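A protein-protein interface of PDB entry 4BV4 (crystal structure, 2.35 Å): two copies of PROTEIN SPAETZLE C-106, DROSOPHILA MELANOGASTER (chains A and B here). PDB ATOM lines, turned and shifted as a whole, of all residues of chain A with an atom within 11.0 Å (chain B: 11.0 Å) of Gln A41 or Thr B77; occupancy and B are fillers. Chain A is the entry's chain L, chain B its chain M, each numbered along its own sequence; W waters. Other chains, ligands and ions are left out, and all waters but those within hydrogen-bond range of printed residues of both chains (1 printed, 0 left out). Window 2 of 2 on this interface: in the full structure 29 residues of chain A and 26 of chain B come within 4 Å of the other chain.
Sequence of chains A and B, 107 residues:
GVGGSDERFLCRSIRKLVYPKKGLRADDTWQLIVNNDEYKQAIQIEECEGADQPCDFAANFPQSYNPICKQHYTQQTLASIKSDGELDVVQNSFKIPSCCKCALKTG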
ATOM      1  N   ARG A  15      15.205 -33.997 -19.347  1.00  0.00           N
ATOM      2  CA  ARG A  15      15.724 -33.319 -18.170  1.00  0.00           C
ATOM      3  C   ARG A  15      15.454 -31.839 -18.319  1.00  0.00           C
ATOM      4  O   ARG A  15      15.829 -31.237 -19.327  1.00  0.00           O
ATOM      5  CB  ARG A  15      17.216 -33.595 -17.945  1.00  0.00           C
ATOM      6  CG  ARG A  15      17.487 -34.905 -17.230  1.00  0.00           C
ATOM      7  CD  ARG A  15      18.452 -34.709 -16.083  1.00  0.00           C
ATOM      8  NE  ARG A  15      18.605 -35.928 -15.291  1.00  0.00           N
ATOM      9  CZ  ARG A  15      18.049 -36.131 -14.101  1.00  0.00           C
ATOM     10  NH1 ARG A  15      17.304 -35.186 -13.538  1.00  0.00           N
ATOM     11  NH2 ARG A  15      18.242 -37.275 -13.459  1.00  0.00           N
ATOM     12  N   LYS A  16      14.735 -31.273 -17.345  1.00  0.00           N
ATOM     13  CA  LYS A  16      14.382 -29.862 -17.295  1.00  0.00           C
ATOM     14  C   LYS A  16      14.445 -29.345 -15.855  1.00  0.00           C
ATOM     15  O   LYS A  16      14.488 -30.117 -14.891  1.00  0.00           O
ATOM     16  CB  LYS A  16      12.999 -29.586 -17.938  1.00  0.00           C
ATOM     17  CG  LYS A  16      11.804 -30.272 -17.269  1.00  0.00           C
ATOM     18  CD  LYS A  16      10.463 -29.693 -17.731  1.00  0.00           C
ATOM     19  CE  LYS A  16       9.944 -28.604 -16.816  1.00  0.00           C
ATOM     20  NZ  LYS A  16       8.456 -28.563 -16.767  1.00  0.00           N
ATOM     21  N   LEU A  17      14.496 -28.023 -15.731  1.00  0.00           N
ATOM     22  CA  LEU A  17      14.549 -27.297 -14.475  1.00  0.00           C
ATOM     23  C   LEU A  17      13.157 -26.831 -14.079  1.00  0.00           C
ATOM     24  O   LEU A  17      12.435 -26.292 -14.917  1.00  0.00           O
ATOM     25  CB  LEU A  17      15.491 -26.073 -14.588  1.00  0.00           C
ATOM     26  CG  LEU A  17      16.991 -26.328 -14.720  1.00  0.00           C
ATOM     27  CD1 LEU A  17      17.722 -25.028 -14.997  1.00  0.00           C
ATOM     28  CD2 LEU A  17      17.560 -26.967 -13.467  1.00  0.00           C
ATOM     29  N   VAL A  18      12.776 -27.043 -12.810  1.00  0.00           N
ATOM     30  CA  VAL A  18      11.481 -26.596 -12.272  1.00  0.00           C
ATOM     31  C   VAL A  18      11.762 -25.590 -11.149  1.00  0.00           C
ATOM     32  O   VAL A  18      12.809 -25.675 -10.489  1.00  0.00           O
ATOM     33  CB  VAL A  18      10.507 -27.735 -11.842  1.00  0.00           C
ATOM     34  CG1 VAL A  18      10.051 -28.550 -13.048  1.00  0.00           C
ATOM     35  CG2 VAL A  18      11.116 -28.647 -10.779  1.00  0.00           C
ATOM     36  N   TYR A  19      10.862 -24.620 -10.967  1.00  0.00           N
ATOM     37  CA  TYR A  19      11.082 -23.557  -9.996  1.00  0.00           C
ATOM     38  C   TYR A  19       9.967 -23.448  -8.947  1.00  0.00           C
ATOM     39  O   TYR A  19       8.914 -22.868  -9.222  1.00  0.00           O
ATOM     40  CB  TYR A  19      11.262 -22.205 -10.727  1.00  0.00           C
ATOM     41  CG  TYR A  19      12.332 -22.228 -11.803  1.00  0.00           C
ATOM     42  CD1 TYR A  19      12.031 -22.620 -13.106  1.00  0.00           C
ATOM     43  CD2 TYR A  19      13.644 -21.851 -11.521  1.00  0.00           C
ATOM     44  CE1 TYR A  19      13.009 -22.643 -14.098  1.00  0.00           C
ATOM     45  CE2 TYR A  19      14.628 -21.860 -12.506  1.00  0.00           C
ATOM     46  CZ  TYR A  19      14.306 -22.255 -13.793  1.00  0.00           C
ATOM     47  OH  TYR A  19      15.276 -22.260 -14.768  1.00  0.00           O
ATOM     48  N   PRO A  20      10.199 -23.969  -7.717  1.00  0.00           N
ATOM     49  CA  PRO A  20       9.203 -23.794  -6.647  1.00  0.00           C
ATOM     50  C   PRO A  20       9.204 -22.335  -6.195  1.00  0.00           C
ATOM     51  O   PRO A  20      10.280 -21.760  -6.006  1.00  0.00           O
ATOM     52  CB  PRO A  20       9.685 -24.751  -5.535  1.00  0.00           C
ATOM     53  CG  PRO A  20      10.847 -25.485  -6.099  1.00  0.00           C
ATOM     54  CD  PRO A  20      11.392 -24.679  -7.215  1.00  0.00           C
ATOM     55  N   LYS A  21       8.007 -21.722  -6.092  1.00  0.00           N
ATOM     56  CA  LYS A  21       7.827 -20.312  -5.728  1.00  0.00           C
ATOM     57  C   LYS A  21       7.071 -20.189  -4.413  1.00  0.00           C
ATOM     58  O   LYS A  21       5.970 -20.726  -4.292  1.00  0.00           O
ATOM     59  CB  LYS A  21       7.072 -19.562  -6.843  1.00  0.00           C
ATOM     60  CG  LYS A  21       7.785 -19.530  -8.195  1.00  0.00           C
ATOM     61  CD  LYS A  21       8.692 -18.314  -8.372  1.00  0.00           C
ATOM     62  CE  LYS A  21       7.963 -17.091  -8.870  1.00  0.00           C
ATOM     63  NZ  LYS A  21       8.891 -15.950  -9.059  1.00  0.00           N
ATOM     64  N   GLN A  41      14.545 -21.552  -5.317  1.00  0.00           N
ATOM     65  CA  GLN A  41      15.710 -21.966  -6.103  1.00  0.00           C
ATOM     66  C   GLN A  41      15.377 -23.192  -7.000  1.00  0.00           C
ATOM     67  O   GLN A  41      14.552 -24.027  -6.626  1.00  0.00           O
ATOM     68  CB  GLN A  41      16.910 -22.260  -5.182  1.00  0.00           C
ATOM     69  CG  GLN A  41      17.454 -21.022  -4.454  1.00  0.00           C
ATOM     70  CD  GLN A  41      18.684 -21.296  -3.607  1.00  0.00           C
ATOM     71  OE1 GLN A  41      19.780 -20.795  -3.883  1.00  0.00           O
ATOM     72  NE2 GLN A  41      18.529 -22.053  -2.527  1.00  0.00           N
ATOM     73  N   ALA A  42      16.051 -23.286  -8.169  1.00  0.00           N
ATOM     74  CA  ALA A  42      15.911 -24.277  -9.248  1.00  0.00           C
ATOM     75  C   ALA A  42      16.219 -25.723  -8.845  1.00  0.00           C
ATOM     76  O   ALA A  42      17.086 -25.953  -8.008  1.00  0.00           O
ATOM     77  CB  ALA A  42      16.828 -23.887 -10.383  1.00  0.00           C
ATOM     78  N   ILE A  43      15.535 -26.705  -9.499  1.00  0.00           N
ATOM     79  CA  ILE A  43      15.703 -28.153  -9.276  1.00  0.00           C
ATOM     80  C   ILE A  43      15.692 -28.913 -10.628  1.00  0.00           C
ATOM     81  O   ILE A  43      14.680 -28.858 -11.335  1.00  0.00           O
ATOM     82  CB  ILE A  43      14.636 -28.752  -8.304  1.00  0.00           C
ATOM     83  CG1 ILE A  43      14.515 -27.950  -6.985  1.00  0.00           C
ATOM     84  CG2 ILE A  43      14.941 -30.224  -8.022  1.00  0.00           C
ATOM     85  CD1 ILE A  43      13.312 -28.286  -6.110  1.00  0.00           C
ATOM     86  N   GLN A  44      16.791 -29.638 -10.973  1.00  0.00           N
ATOM     87  CA  GLN A  44      16.843 -30.414 -12.220  1.00  0.00           C
ATOM     88  C   GLN A  44      16.072 -31.727 -12.024  1.00  0.00           C
ATOM     89  O   GLN A  44      16.372 -32.531 -11.137  1.00  0.00           O
ATOM     90  CB  GLN A  44      18.274 -30.652 -12.733  1.00  0.00           C
ATOM     91  CG  GLN A  44      18.296 -31.136 -14.190  1.00  0.00           C
ATOM     92  CD  GLN A  44      19.684 -31.277 -14.762  1.00  0.00           C
ATOM     93  OE1 GLN A  44      20.491 -32.099 -14.312  1.00  0.00           O
ATOM     94  NE2 GLN A  44      19.971 -30.513 -15.809  1.00  0.00           N
ATOM     95  N   ILE A  45      15.081 -31.918 -12.885  1.00  0.00           N
ATOM     96  CA  ILE A  45      14.073 -32.956 -12.840  1.00  0.00           C
ATOM     97  C   ILE A  45      14.021 -33.787 -14.125  1.00  0.00           C
ATOM     98  O   ILE A  45      14.650 -33.437 -15.121  1.00  0.00           O
ATOM     99  CB  ILE A  45      12.759 -32.122 -12.606  1.00  0.00           C
ATOM    100  CG1 ILE A  45      12.079 -32.455 -11.319  1.00  0.00           C
ATOM    101  CG2 ILE A  45      11.794 -31.912 -13.815  1.00  0.00           C
ATOM    102  CD1 ILE A  45      12.813 -31.999 -10.161  1.00  0.00           C
ATOM    103  N   GLN A  76       8.359 -31.757  -1.175  1.00  0.00           N
ATOM    104  CA  GLN A  76       9.344 -30.999  -0.415  1.00  0.00           C
ATOM    105  C   GLN A  76       8.585 -29.928   0.344  1.00  0.00           C
ATOM    106  O   GLN A  76       7.649 -29.353  -0.210  1.00  0.00           O
ATOM    107  CB  GLN A  76      10.435 -30.411  -1.331  1.00  0.00           C
ATOM    108  CG  GLN A  76      11.293 -31.506  -2.001  1.00  0.00           C
ATOM    109  CD  GLN A  76      12.612 -31.036  -2.581  1.00  0.00           C
ATOM    110  OE1 GLN A  76      13.063 -29.901  -2.361  1.00  0.00           O
ATOM    111  NE2 GLN A  76      13.281 -31.922  -3.317  1.00  0.00           N
ATOM    112  N   PHE A  94       5.478 -28.520  -1.781  1.00  0.00           N
ATOM    113  CA  PHE A  94       5.593 -28.454  -3.239  1.00  0.00           C
ATOM    114  C   PHE A  94       5.605 -29.852  -3.822  1.00  0.00           C
ATOM    115  O   PHE A  94       6.394 -30.701  -3.381  1.00  0.00           O
ATOM    116  CB  PHE A  94       6.863 -27.689  -3.667  1.00  0.00           C
ATOM    117  CG  PHE A  94       6.931 -26.247  -3.201  1.00  0.00           C
ATOM    118  CD1 PHE A  94       7.498 -25.920  -1.971  1.00  0.00           C
ATOM    119  CD2 PHE A  94       6.429 -25.219  -3.992  1.00  0.00           C
ATOM    120  CE1 PHE A  94       7.553 -24.592  -1.539  1.00  0.00           C
ATOM    121  CE2 PHE A  94       6.495 -23.890  -3.563  1.00  0.00           C
ATOM    122  CZ  PHE A  94       7.052 -23.585  -2.338  1.00  0.00           C
ATOM    123  N   ILE A  96       6.773 -31.860  -6.593  1.00  0.00           N
ATOM    124  CA  ILE A  96       7.788 -31.694  -7.636  1.00  0.00           C
ATOM    125  C   ILE A  96       7.982 -33.011  -8.434  1.00  0.00           C
ATOM    126  O   ILE A  96       8.136 -34.072  -7.829  1.00  0.00           O
ATOM    127  CB  ILE A  96       9.131 -31.086  -7.082  1.00  0.00           C
ATOM    128  CG1 ILE A  96      10.286 -32.082  -6.975  1.00  0.00           C
ATOM    129  CG2 ILE A  96       8.943 -30.218  -5.787  1.00  0.00           C
ATOM    130  CD1 ILE A  96      11.613 -31.471  -6.824  1.00  0.00           C
ATOM    131  N   ILE B  43      12.298 -33.205   3.046  1.00  0.00           N
ATOM    132  CA  ILE B  43      12.340 -33.534   1.620  1.00  0.00           C
ATOM    133  C   ILE B  43      12.185 -35.059   1.494  1.00  0.00           C
ATOM    134  O   ILE B  43      12.843 -35.812   2.217  1.00  0.00           O
ATOM    135  CB  ILE B  43      13.553 -32.942   0.824  1.00  0.00           C
ATOM    136  CG1 ILE B  43      14.888 -33.572   1.189  1.00  0.00           C
ATOM    137  CG2 ILE B  43      13.635 -31.412   0.914  1.00  0.00           C
ATOM    138  CD1 ILE B  43      15.462 -34.283   0.041  1.00  0.00           C
ATOM    139  N   TYR B  73      18.405 -39.573  -9.533  1.00  0.00           N
ATOM    140  CA  TYR B  73      18.665 -38.419  -8.678  1.00  0.00           C
ATOM    141  C   TYR B  73      18.124 -37.133  -9.281  1.00  0.00           C
ATOM    142  O   TYR B  73      18.124 -36.978 -10.505  1.00  0.00           O
ATOM    143  CB  TYR B  73      20.172 -38.253  -8.431  1.00  0.00           C
ATOM    144  CG  TYR B  73      20.803 -39.406  -7.686  1.00  0.00           C
ATOM    145  CD1 TYR B  73      20.800 -39.447  -6.294  1.00  0.00           C
ATOM    146  CD2 TYR B  73      21.451 -40.432  -8.368  1.00  0.00           C
ATOM    147  CE1 TYR B  73      21.387 -40.504  -5.599  1.00  0.00           C
ATOM    148  CE2 TYR B  73      22.054 -41.488  -7.684  1.00  0.00           C
ATOM    149  CZ  TYR B  73      22.025 -41.516  -6.300  1.00  0.00           C
ATOM    150  OH  TYR B  73      22.619 -42.549  -5.620  1.00  0.00           O
ATOM    151  N   THR B  74      17.685 -36.208  -8.416  1.00  0.00           N
ATOM    152  CA  THR B  74      17.245 -34.874  -8.802  1.00  0.00           C
ATOM    153  C   THR B  74      18.267 -33.909  -8.200  1.00  0.00           C
ATOM    154  O   THR B  74      18.700 -34.124  -7.065  1.00  0.00           O
ATOM    155  CB  THR B  74      15.783 -34.593  -8.394  1.00  0.00           C
ATOM    156  OG1 THR B  74      15.589 -34.882  -7.015  1.00  0.00           O
ATOM    157  CG2 THR B  74      14.775 -35.366  -9.233  1.00  0.00           C
ATOM    158  N   GLN B  75      18.714 -32.904  -8.970  1.00  0.00           N
ATOM    159  CA  GLN B  75      19.720 -31.961  -8.483  1.00  0.00           C
ATOM    160  C   GLN B  75      19.077 -30.669  -7.998  1.00  0.00           C
ATOM    161  O   GLN B  75      18.249 -30.092  -8.696  1.00  0.00           O
ATOM    162  CB  GLN B  75      20.777 -31.662  -9.553  1.00  0.00           C
ATOM    163  CG  GLN B  75      21.884 -32.708  -9.618  1.00  0.00           C
ATOM    164  CD  GLN B  75      22.913 -32.365 -10.669  1.00  0.00           C
ATOM    165  OE1 GLN B  75      23.764 -31.486 -10.479  1.00  0.00           O
ATOM    166  NE2 GLN B  75      22.861 -33.056 -11.800  1.00  0.00           N
ATOM    167  N   GLN B  76      19.473 -30.218  -6.808  1.00  0.00           N
ATOM    168  CA  GLN B  76      18.968 -28.995  -6.205  1.00  0.00           C
ATOM    169  C   GLN B  76      20.017 -27.874  -6.254  1.00  0.00           C
ATOM    170  O   GLN B  76      21.203 -28.125  -5.998  1.00  0.00           O
ATOM    171  CB  GLN B  76      18.521 -29.257  -4.763  1.00  0.00           C
ATOM    172  CG  GLN B  76      17.063 -29.681  -4.687  1.00  0.00           C
ATOM    173  CD  GLN B  76      16.320 -28.932  -3.613  1.00  0.00           C
ATOM    174  OE1 GLN B  76      16.149 -27.709  -3.667  1.00  0.00           O
ATOM    175  NE2 GLN B  76      15.840 -29.656  -2.620  1.00  0.00           N
ATOM    176  N   THR B  77      19.562 -26.642  -6.597  1.00  0.00           N
ATOM    177  CA  THR B  77      20.364 -25.415  -6.702  1.00  0.00           C
ATOM    178  C   THR B  77      19.888 -24.418  -5.641  1.00  0.00           C
ATOM    179  O   THR B  77      20.706 -23.813  -4.951  1.00  0.00           O
ATOM    180  CB  THR B  77      20.270 -24.823  -8.130  1.00  0.00           C
ATOM    181  OG1 THR B  77      20.584 -25.831  -9.095  1.00  0.00           O
ATOM    182  CG2 THR B  77      21.183 -23.621  -8.337  1.00  0.00           C
ATOM    183  N   PHE B  94      23.047 -30.029  -5.044  1.00  0.00           N
ATOM    184  CA  PHE B  94      23.270 -31.356  -4.465  1.00  0.00           C
ATOM    185  C   PHE B  94      22.242 -32.390  -4.979  1.00  0.00           C
ATOM    186  O   PHE B  94      21.136 -32.020  -5.383  1.00  0.00           O
ATOM    187  CB  PHE B  94      23.274 -31.309  -2.921  1.00  0.00           C
ATOM    188  CG  PHE B  94      22.074 -30.652  -2.283  1.00  0.00           C
ATOM    189  CD1 PHE B  94      20.943 -31.393  -1.967  1.00  0.00           C
ATOM    190  CD2 PHE B  94      22.084 -29.297  -1.979  1.00  0.00           C
ATOM    191  CE1 PHE B  94      19.828 -30.783  -1.381  1.00  0.00           C
ATOM    192  CE2 PHE B  94      20.970 -28.686  -1.390  1.00  0.00           C
ATOM    193  CZ  PHE B  94      19.850 -29.435  -1.091  1.00  0.00           C
ATOM    194  N   LYS B  95      22.621 -33.690  -4.943  1.00  0.00           N
ATOM    195  CA  LYS B  95      21.809 -34.808  -5.432  1.00  0.00           C
ATOM    196  C   LYS B  95      20.869 -35.369  -4.371  1.00  0.00           C
ATOM    197  O   LYS B  95      21.238 -35.481  -3.206  1.00  0.00           O
ATOM    198  CB  LYS B  95      22.704 -35.931  -5.976  1.00  0.00           C
ATOM    199  CG  LYS B  95      23.235 -35.640  -7.372  1.00  0.00           C
ATOM    200  CD  LYS B  95      24.471 -36.467  -7.698  1.00  0.00           C
ATOM    201  CE  LYS B  95      25.134 -36.021  -8.983  1.00  0.00           C
ATOM    202  NZ  LYS B  95      25.748 -34.666  -8.869  1.00  0.00           N
ATOM    203  N   ILE B  96      19.651 -35.729  -4.796  1.00  0.00           N
ATOM    204  CA  ILE B  96      18.603 -36.315  -3.959  1.00  0.00           C
ATOM    205  C   ILE B  96      18.115 -37.612  -4.630  1.00  0.00           C
ATOM    206  O   ILE B  96      17.679 -37.545  -5.781  1.00  0.00           O
ATOM    207  CB  ILE B  96      17.444 -35.295  -3.727  1.00  0.00           C
ATOM    208  CG1 ILE B  96      17.890 -34.170  -2.767  1.00  0.00           C
ATOM    209  CG2 ILE B  96      16.162 -35.977  -3.212  1.00  0.00           C
ATOM    210  CD1 ILE B  96      17.242 -32.860  -3.013  1.00  0.00           C
HETATM  211  O   HOH W   1      20.109 -39.409 -12.096  1.00  0.00           O
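O of Tyr B73 is in hydrogen-bond range of NH2 of Arg A15.
The side-chain amide oxygen (OE1) of Gln A41 sits close to the backbone carbonyl oxygen (O) of Thr B77 (3.3 Å).
O of Ala A42 lies within hydrogen-bond range of N of Thr B77 (2.9 Å).
N of Gln A44 is in hydrogen-bond range of O of Gln B75 (2.7 Å).
The side-chain amide oxygen (OE1) of Gln A76 lies within hydrogen-bond range of the side-chain amide nitrogen (NE2) of Gln B76.
N of Val A18 lies within hydrogen-bond range of O of Ile A43.
O of Gln A76 sits at hydrogen-bond distance from N of Phe A94 (2.8 Å).
The backbone NH (N) of Ile B96 is in hydrogen-bond range of the backbone carbonyl oxygen (O) of Thr B74 (2.9 Å).
The backbone NH of Phe B94 is in hydrogen-bond range of the backbone carbonyl oxygen of Gln B76.
Among the printed residues, pairs that only touch across the chains: Ile A43 with Gln B75, Gln A44 with Thr B74, Gln A76 with Ile B43, Ile A43 with Gln B76 and Ala A42 with Gln B76.
Gln A41 touches just one residue of chain B: Thr B77 (3.3 Å).
Of chain A, only Gln A41 and Ala A42 come within 4 Å of Thr B77.
No residue of chain B comes within 4 Å of Pro A20.
Of chain B, only Gln B75 (3.3 Å) and Gln B76 (3.7 Å) come within 4 Å of Ile A43.
Of the printed residues of chain A, Tyr B73 touches Arg A15.
Printed residues of chain A within 4 Å of Ile B43: Gln A76.
Lys B95 touches none of the printed residues of chain A.
Ile A96 touches none of the printed residues of chain B.
The nearest residue of chain A that does not touch Thr B77 is Ile A43 (4.9 Å).
The nearest printed residue of chain B that does not touch Arg A15 is Thr B74 (4.7 Å).
Of the 15 printed residues of chain A, 6 touch a printed residue of chain B.
Along chain A the printed residues that touch a printed residue of chain B span positions 15 to 76.
Ile A43 touches Gln B76, and with the chains exchanged Gln A76 touches Ile B43.
Gln A76 touches its own counterpart, Gln B76.
Positions printed for both chains: 43, 76, 94 and 96.
Of the 10 pairs that touch across the chains among the printed residues, 3 have their exchanged pair printed and touching as well.
Water W1 lies within hydrogen-bond range of the backbone NH (N) of Tyr B73 (3.1 Å) and the guanidinium group (NH2) of Arg A15 (3.1 Å).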
